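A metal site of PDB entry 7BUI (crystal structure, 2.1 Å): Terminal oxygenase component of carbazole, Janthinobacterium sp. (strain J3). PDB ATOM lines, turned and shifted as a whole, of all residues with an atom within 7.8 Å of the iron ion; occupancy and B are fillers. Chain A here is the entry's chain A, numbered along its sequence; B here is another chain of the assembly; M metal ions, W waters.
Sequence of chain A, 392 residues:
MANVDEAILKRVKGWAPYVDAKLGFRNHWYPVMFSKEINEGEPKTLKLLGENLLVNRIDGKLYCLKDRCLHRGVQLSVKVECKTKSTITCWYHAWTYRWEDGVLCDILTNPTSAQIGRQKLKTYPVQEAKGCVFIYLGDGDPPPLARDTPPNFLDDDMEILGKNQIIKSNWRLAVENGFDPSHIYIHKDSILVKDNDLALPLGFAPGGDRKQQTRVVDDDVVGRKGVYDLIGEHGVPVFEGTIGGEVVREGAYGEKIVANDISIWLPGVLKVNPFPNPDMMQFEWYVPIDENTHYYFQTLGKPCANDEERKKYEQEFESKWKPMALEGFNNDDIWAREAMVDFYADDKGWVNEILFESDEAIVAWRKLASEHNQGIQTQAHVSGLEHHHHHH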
ATOM      1  N   ASN A 177      29.155 -14.978  25.891  1.00  0.00           N
ATOM      2  CA  ASN A 177      28.822 -15.600  24.590  1.00  0.00           C
ATOM      3  C   ASN A 177      30.026 -15.375  23.637  1.00  0.00           C
ATOM      4  O   ASN A 177      30.436 -16.334  23.019  1.00  0.00           O
ATOM      5  CB  ASN A 177      27.520 -15.068  23.986  1.00  0.00           C
ATOM      6  CG  ASN A 177      27.278 -15.670  22.628  1.00  0.00           C
ATOM      7  OD1 ASN A 177      26.922 -16.849  22.520  1.00  0.00           O
ATOM      8  ND2 ASN A 177      27.595 -14.909  21.582  1.00  0.00           N
ATOM      9  N   GLY A 178      30.592 -14.162  23.600  1.00  0.00           N
ATOM     10  CA  GLY A 178      31.762 -13.795  22.780  1.00  0.00           C
ATOM     11  C   GLY A 178      32.940 -14.713  23.043  1.00  0.00           C
ATOM     12  O   GLY A 178      33.515 -15.248  22.085  1.00  0.00           O
ATOM     13  N   PHE A 179      33.249 -14.947  24.315  1.00  0.00           N
ATOM     14  CA  PHE A 179      34.515 -15.562  24.772  1.00  0.00           C
ATOM     15  C   PHE A 179      34.312 -17.069  24.922  1.00  0.00           C
ATOM     16  O   PHE A 179      35.228 -17.772  25.368  1.00  0.00           O
ATOM     17  CB  PHE A 179      35.006 -14.881  26.051  1.00  0.00           C
ATOM     18  CG  PHE A 179      36.396 -15.265  26.443  1.00  0.00           C
ATOM     19  CD1 PHE A 179      37.451 -15.109  25.543  1.00  0.00           C
ATOM     20  CD2 PHE A 179      36.662 -15.796  27.693  1.00  0.00           C
ATOM     21  CE1 PHE A 179      38.745 -15.471  25.903  1.00  0.00           C
ATOM     22  CE2 PHE A 179      37.952 -16.174  28.039  1.00  0.00           C
ATOM     23  CZ  PHE A 179      38.994 -16.000  27.147  1.00  0.00           C
ATOM     24  N   ASP A 180      33.139 -17.559  24.551  1.00  0.00           N
ATOM     25  CA  ASP A 180      32.721 -18.946  24.847  1.00  0.00           C
ATOM     26  C   ASP A 180      33.253 -19.880  23.756  1.00  0.00           C
ATOM     27  O   ASP A 180      32.745 -19.870  22.635  1.00  0.00           O
ATOM     28  CB  ASP A 180      31.197 -19.011  24.944  1.00  0.00           C
ATOM     29  CG  ASP A 180      30.642 -20.369  25.321  1.00  0.00           C
ATOM     30  OD1 ASP A 180      31.387 -21.372  25.165  1.00  0.00           O
ATOM     31  OD2 ASP A 180      29.470 -20.398  25.787  1.00  0.00           O
ATOM     32  N   HIS A 183      30.660 -22.135  21.862  1.00  0.00           N
ATOM     33  CA  HIS A 183      29.463 -21.443  21.297  1.00  0.00           C
ATOM     34  C   HIS A 183      29.544 -21.451  19.766  1.00  0.00           C
ATOM     35  O   HIS A 183      28.548 -21.081  19.165  1.00  0.00           O
ATOM     36  CB  HIS A 183      29.330 -20.017  21.835  1.00  0.00           C
ATOM     37  CG  HIS A 183      29.917 -18.953  20.965  1.00  0.00           C
ATOM     38  ND1 HIS A 183      31.249 -18.565  21.060  1.00  0.00           N
ATOM     39  CD2 HIS A 183      29.359 -18.157  20.021  1.00  0.00           C
ATOM     40  CE1 HIS A 183      31.486 -17.590  20.179  1.00  0.00           C
ATOM     41  NE2 HIS A 183      30.352 -17.319  19.525  1.00  0.00           N
ATOM     42  N   ILE A 184      30.691 -21.819  19.189  1.00  0.00           N
ATOM     43  CA  ILE A 184      30.890 -21.821  17.708  1.00  0.00           C
ATOM     44  C   ILE A 184      29.844 -22.718  17.041  1.00  0.00           C
ATOM     45  O   ILE A 184      29.461 -22.414  15.914  1.00  0.00           O
ATOM     46  CB  ILE A 184      32.320 -22.215  17.287  1.00  0.00           C
ATOM     47  CG1 ILE A 184      32.739 -23.583  17.825  1.00  0.00           C
ATOM     48  CG2 ILE A 184      33.305 -21.123  17.715  1.00  0.00           C
ATOM     49  CD1 ILE A 184      34.108 -24.027  17.329  1.00  0.00           C
ATOM     50  N   ILE A 186      26.801 -22.481  17.183  1.00  0.00           N
ATOM     51  CA  ILE A 186      25.663 -21.653  16.688  1.00  0.00           C
ATOM     52  C   ILE A 186      25.989 -21.063  15.302  1.00  0.00           C
ATOM     53  O   ILE A 186      25.026 -20.621  14.650  1.00  0.00           O
ATOM     54  CB  ILE A 186      25.248 -20.525  17.668  1.00  0.00           C
ATOM     55  CG1 ILE A 186      26.292 -19.408  17.727  1.00  0.00           C
ATOM     56  CG2 ILE A 186      24.907 -21.080  19.036  1.00  0.00           C
ATOM     57  CD1 ILE A 186      25.907 -18.244  18.581  1.00  0.00           C
ATOM     58  N   HIS A 187      27.271 -20.988  14.925  1.00  0.00           N
ATOM     59  CA  HIS A 187      27.756 -20.321  13.679  1.00  0.00           C
ATOM     60  C   HIS A 187      27.849 -21.313  12.518  1.00  0.00           C
ATOM     61  O   HIS A 187      28.239 -20.911  11.406  1.00  0.00           O
ATOM     62  CB  HIS A 187      29.099 -19.638  13.941  1.00  0.00           C
ATOM     63  CG  HIS A 187      28.959 -18.456  14.851  1.00  0.00           C
ATOM     64  ND1 HIS A 187      28.009 -17.475  14.636  1.00  0.00           N
ATOM     65  CD2 HIS A 187      29.616 -18.126  15.996  1.00  0.00           C
ATOM     66  CE1 HIS A 187      28.109 -16.568  15.593  1.00  0.00           C
ATOM     67  NE2 HIS A 187      29.084 -16.951  16.439  1.00  0.00           N
ATOM     68  N   LEU A 270      36.211  -7.950  23.395  1.00  0.00           N
ATOM     69  CA  LEU A 270      36.736  -9.184  22.798  1.00  0.00           C
ATOM     70  C   LEU A 270      37.618  -8.763  21.605  1.00  0.00           C
ATOM     71  O   LEU A 270      37.224  -7.842  20.856  1.00  0.00           O
ATOM     72  CB  LEU A 270      35.569 -10.031  22.324  1.00  0.00           C
ATOM     73  CG  LEU A 270      35.926 -11.467  21.943  1.00  0.00           C
ATOM     74  CD1 LEU A 270      35.949 -12.376  23.164  1.00  0.00           C
ATOM     75  CD2 LEU A 270      34.944 -12.009  20.950  1.00  0.00           C
ATOM     76  N   PHE A 275      40.228 -12.229  11.977  1.00  0.00           N
ATOM     77  CA  PHE A 275      38.772 -12.369  11.724  1.00  0.00           C
ATOM     78  C   PHE A 275      38.228 -11.131  11.025  1.00  0.00           C
ATOM     79  O   PHE A 275      38.640 -10.019  11.349  1.00  0.00           O
ATOM     80  CB  PHE A 275      37.988 -12.646  13.018  1.00  0.00           C
ATOM     81  CG  PHE A 275      36.693 -13.391  12.775  1.00  0.00           C
ATOM     82  CD1 PHE A 275      36.694 -14.762  12.631  1.00  0.00           C
ATOM     83  CD2 PHE A 275      35.493 -12.706  12.641  1.00  0.00           C
ATOM     84  CE1 PHE A 275      35.516 -15.445  12.345  1.00  0.00           C
ATOM     85  CE2 PHE A 275      34.316 -13.386  12.372  1.00  0.00           C
ATOM     86  CZ  PHE A 275      34.334 -14.748  12.213  1.00  0.00           C
ATOM     87  N   GLU A 284      35.397  -6.201  19.612  1.00  0.00           N
ATOM     88  CA  GLU A 284      33.989  -5.846  19.927  1.00  0.00           C
ATOM     89  C   GLU A 284      33.800  -5.626  21.419  1.00  0.00           C
ATOM     90  O   GLU A 284      34.342  -6.409  22.237  1.00  0.00           O
ATOM     91  CB  GLU A 284      32.981  -6.827  19.309  1.00  0.00           C
ATOM     92  CG  GLU A 284      33.191  -8.284  19.649  1.00  0.00           C
ATOM     93  CD  GLU A 284      32.125  -9.167  19.034  1.00  0.00           C
ATOM     94  OE1 GLU A 284      31.728  -8.892  17.902  1.00  0.00           O
ATOM     95  OE2 GLU A 284      31.663 -10.115  19.702  1.00  0.00           O
ATOM     96  N   TYR A 286      31.021  -4.787  24.668  1.00  0.00           N
ATOM     97  CA  TYR A 286      29.674  -5.026  25.228  1.00  0.00           C
ATOM     98  C   TYR A 286      29.492  -4.014  26.350  1.00  0.00           C
ATOM     99  O   TYR A 286      29.914  -4.279  27.478  1.00  0.00           O
ATOM    100  CB  TYR A 286      29.556  -6.490  25.652  1.00  0.00           C
ATOM    101  CG  TYR A 286      30.209  -7.472  24.704  1.00  0.00           C
ATOM    102  CD1 TYR A 286      29.569  -7.904  23.571  1.00  0.00           C
ATOM    103  CD2 TYR A 286      31.453  -7.996  24.980  1.00  0.00           C
ATOM    104  CE1 TYR A 286      30.137  -8.858  22.735  1.00  0.00           C
ATOM    105  CE2 TYR A 286      32.060  -8.912  24.146  1.00  0.00           C
ATOM    106  CZ  TYR A 286      31.396  -9.340  23.014  1.00  0.00           C
ATOM    107  OH  TYR A 286      31.996 -10.261  22.223  1.00  0.00           O
ATOM    108  N   TYR A 296      26.238  -3.062  21.432  1.00  0.00           N
ATOM    109  CA  TYR A 296      27.091  -4.055  20.724  1.00  0.00           C
ATOM    110  C   TYR A 296      27.930  -3.245  19.726  1.00  0.00           C
ATOM    111  O   TYR A 296      27.505  -3.020  18.576  1.00  0.00           O
ATOM    112  CB  TYR A 296      26.247  -5.180  20.122  1.00  0.00           C
ATOM    113  CG  TYR A 296      27.053  -6.263  19.441  1.00  0.00           C
ATOM    114  CD1 TYR A 296      28.295  -6.635  19.889  1.00  0.00           C
ATOM    115  CD2 TYR A 296      26.536  -6.946  18.347  1.00  0.00           C
ATOM    116  CE1 TYR A 296      29.031  -7.629  19.267  1.00  0.00           C
ATOM    117  CE2 TYR A 296      27.269  -7.923  17.699  1.00  0.00           C
ATOM    118  CZ  TYR A 296      28.520  -8.271  18.165  1.00  0.00           C
ATOM    119  OH  TYR A 296      29.234  -9.271  17.534  1.00  0.00           O
ATOM    120  N   PHE A 329      27.329 -13.162  10.400  1.00  0.00           N
ATOM    121  CA  PHE A 329      27.948 -14.107  11.379  1.00  0.00           C
ATOM    122  C   PHE A 329      27.482 -13.764  12.803  1.00  0.00           C
ATOM    123  O   PHE A 329      27.012 -14.686  13.484  1.00  0.00           O
ATOM    124  CB  PHE A 329      29.467 -14.095  11.263  1.00  0.00           C
ATOM    125  CG  PHE A 329      30.174 -15.151  12.081  1.00  0.00           C
ATOM    126  CD1 PHE A 329      30.327 -16.442  11.615  1.00  0.00           C
ATOM    127  CD2 PHE A 329      30.691 -14.850  13.341  1.00  0.00           C
ATOM    128  CE1 PHE A 329      31.009 -17.399  12.363  1.00  0.00           C
ATOM    129  CE2 PHE A 329      31.373 -15.807  14.089  1.00  0.00           C
ATOM    130  CZ  PHE A 329      31.531 -17.083  13.591  1.00  0.00           C
ATOM    131  N   ASN A 330      27.608 -12.500  13.235  1.00  0.00           N
ATOM    132  CA  ASN A 330      27.375 -12.058  14.634  1.00  0.00           C
ATOM    133  C   ASN A 330      25.877 -11.966  14.954  1.00  0.00           C
ATOM    134  O   ASN A 330      25.551 -11.959  16.154  1.00  0.00           O
ATOM    135  CB  ASN A 330      28.095 -10.762  14.977  1.00  0.00           C
ATOM    136  CG  ASN A 330      29.602 -10.929  15.049  1.00  0.00           C
ATOM    137  OD1 ASN A 330      30.332 -10.151  14.424  1.00  0.00           O
ATOM    138  ND2 ASN A 330      30.059 -11.943  15.782  1.00  0.00           N
ATOM    139  N   ASN A 331      24.983 -11.940  13.952  1.00  0.00           N
ATOM    140  CA  ASN A 331      23.522 -11.853  14.204  1.00  0.00           C
ATOM    141  C   ASN A 331      23.093 -13.061  15.049  1.00  0.00           C
ATOM    142  O   ASN A 331      22.175 -12.915  15.888  1.00  0.00           O
ATOM    143  CB  ASN A 331      22.681 -11.800  12.940  1.00  0.00           C
ATOM    144  CG  ASN A 331      22.435 -10.378  12.467  1.00  0.00           C
ATOM    145  OD1 ASN A 331      22.837  -9.417  13.121  1.00  0.00           O
ATOM    146  ND2 ASN A 331      21.793 -10.243  11.326  1.00  0.00           N
ATOM    147  N   ASP A 332      23.697 -14.215  14.838  1.00  0.00           N
ATOM    148  CA  ASP A 332      23.365 -15.405  15.667  1.00  0.00           C
ATOM    149  C   ASP A 332      23.807 -15.156  17.120  1.00  0.00           C
ATOM    150  O   ASP A 332      23.171 -15.721  17.999  1.00  0.00           O
ATOM    151  CB  ASP A 332      23.953 -16.686  15.069  1.00  0.00           C
ATOM    152  CG  ASP A 332      23.249 -17.143  13.799  1.00  0.00           C
ATOM    153  OD1 ASP A 332      22.025 -17.020  13.721  1.00  0.00           O
ATOM    154  OD2 ASP A 332      23.942 -17.659  12.917  1.00  0.00           O
ATOM    155  N   ASP A 333      24.860 -14.373  17.373  1.00  0.00           N
ATOM    156  CA  ASP A 333      25.332 -14.072  18.743  1.00  0.00           C
ATOM    157  C   ASP A 333      24.303 -13.208  19.476  1.00  0.00           C
ATOM    158  O   ASP A 333      24.121 -13.392  20.702  1.00  0.00           O
ATOM    159  CB  ASP A 333      26.699 -13.382  18.766  1.00  0.00           C
ATOM    160  CG  ASP A 333      27.842 -14.239  18.260  1.00  0.00           C
ATOM    161  OD1 ASP A 333      28.008 -15.334  18.770  1.00  0.00           O
ATOM    162  OD2 ASP A 333      28.544 -13.799  17.348  1.00  0.00           O
ATOM    163  N   ILE A 334      23.641 -12.289  18.770  1.00  0.00           N
ATOM    164  CA  ILE A 334      22.604 -11.384  19.342  1.00  0.00           C
ATOM    165  C   ILE A 334      21.464 -12.237  19.940  1.00  0.00           C
ATOM    166  O   ILE A 334      21.137 -11.995  21.113  1.00  0.00           O
ATOM    167  CB  ILE A 334      22.107 -10.384  18.296  1.00  0.00           C
ATOM    168  CG1 ILE A 334      23.218  -9.383  17.937  1.00  0.00           C
ATOM    169  CG2 ILE A 334      20.846  -9.692  18.766  1.00  0.00           C
ATOM    170  CD1 ILE A 334      22.843  -8.431  16.815  1.00  0.00           C
ATOM    171  N   ALA A 336      21.413 -15.460  20.625  1.00  0.00           N
ATOM    172  CA  ALA A 336      21.956 -16.394  21.638  1.00  0.00           C
ATOM    173  C   ALA A 336      21.981 -15.710  23.019  1.00  0.00           C
ATOM    174  O   ALA A 336      21.518 -16.307  24.015  1.00  0.00           O
ATOM    175  CB  ALA A 336      23.336 -16.874  21.219  1.00  0.00           C
ATOM    176  N   ARG A 337      22.535 -14.493  23.065  1.00  0.00           N
ATOM    177  CA  ARG A 337      22.588 -13.632  24.264  1.00  0.00           C
ATOM    178  C   ARG A 337      21.172 -13.436  24.798  1.00  0.00           C
ATOM    179  O   ARG A 337      20.988 -13.556  26.013  1.00  0.00           O
ATOM    180  CB  ARG A 337      23.030 -12.207  23.918  1.00  0.00           C
ATOM    181  CG  ARG A 337      24.507 -12.034  23.668  1.00  0.00           C
ATOM    182  CD  ARG A 337      24.747 -10.651  23.079  1.00  0.00           C
ATOM    183  NE  ARG A 337      25.822 -10.804  22.142  1.00  0.00           N
ATOM    184  CZ  ARG A 337      26.299  -9.859  21.362  1.00  0.00           C
ATOM    185  NH1 ARG A 337      25.800  -8.627  21.391  1.00  0.00           N
ATOM    186  NH2 ARG A 337      27.292 -10.172  20.549  1.00  0.00           N
ATOM    187  N   TYR B  92      22.628 -24.291  21.228  1.00  0.00           N
ATOM    188  CA  TYR B  92      23.684 -23.398  21.741  1.00  0.00           C
ATOM    189  C   TYR B  92      25.033 -24.116  21.712  1.00  0.00           C
ATOM    190  O   TYR B  92      25.921 -23.713  20.935  1.00  0.00           O
ATOM    191  CB  TYR B  92      23.318 -22.851  23.130  1.00  0.00           C
ATOM    192  CG  TYR B  92      23.984 -21.562  23.508  1.00  0.00           C
ATOM    193  CD1 TYR B  92      24.982 -20.988  22.720  1.00  0.00           C
ATOM    194  CD2 TYR B  92      23.632 -20.896  24.666  1.00  0.00           C
ATOM    195  CE1 TYR B  92      25.573 -19.787  23.037  1.00  0.00           C
ATOM    196  CE2 TYR B  92      24.221 -19.696  25.013  1.00  0.00           C
ATOM    197  CZ  TYR B  92      25.198 -19.138  24.206  1.00  0.00           C
ATOM    198  OH  TYR B  92      25.807 -17.969  24.558  1.00  0.00           O
HETATM  199 FE    FE M   1      29.861 -15.887  18.166  1.00  0.00          FE
HETATM  200  O   HOH W   1      32.011 -15.408  17.620  1.00  0.00           O
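O of Phe 329 lies close to ND1 of His 187.
The side-chain carboxylate (OD2) of Asp 333 lies within hydrogen-bond range of the side-chain amide nitrogen (ND2) of Asn 330 (2.9 Å).
The backbone carbonyl oxygen of Asp 333 lies close to the guanidinium group of Arg 337 (3.4 Å).
ND1 of His 183 is in hydrogen-bond range of O of Asp 180 (2.5 Å).
The side-chain carboxylate (OD1) of Asp 333 sits close to the side-chain amide nitrogen (ND2) of Asn 177 (2.9 Å).
ND1 of His 183 lies within hydrogen-bond range of O of Asn 177, 3.1 Å away.
Of the 22 residues printed, 3 come within 4 Å of the iron ion.
The nearest printed residue that does not touch the iron ion is Asn 177 (4.2 Å).
The iron ion is bound by the side-chain carboxylate of Asp 333 (2.0 Å), a ring nitrogen (NE2) of His 183 (2.0 Å), a ring nitrogen (NE2) of His 187 (2.2 Å) and water W1 (2.3 Å).
Slightly farther from the iron ion lies the side-chain carboxylate (OD2) of Asp 333 (2.6 Å).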
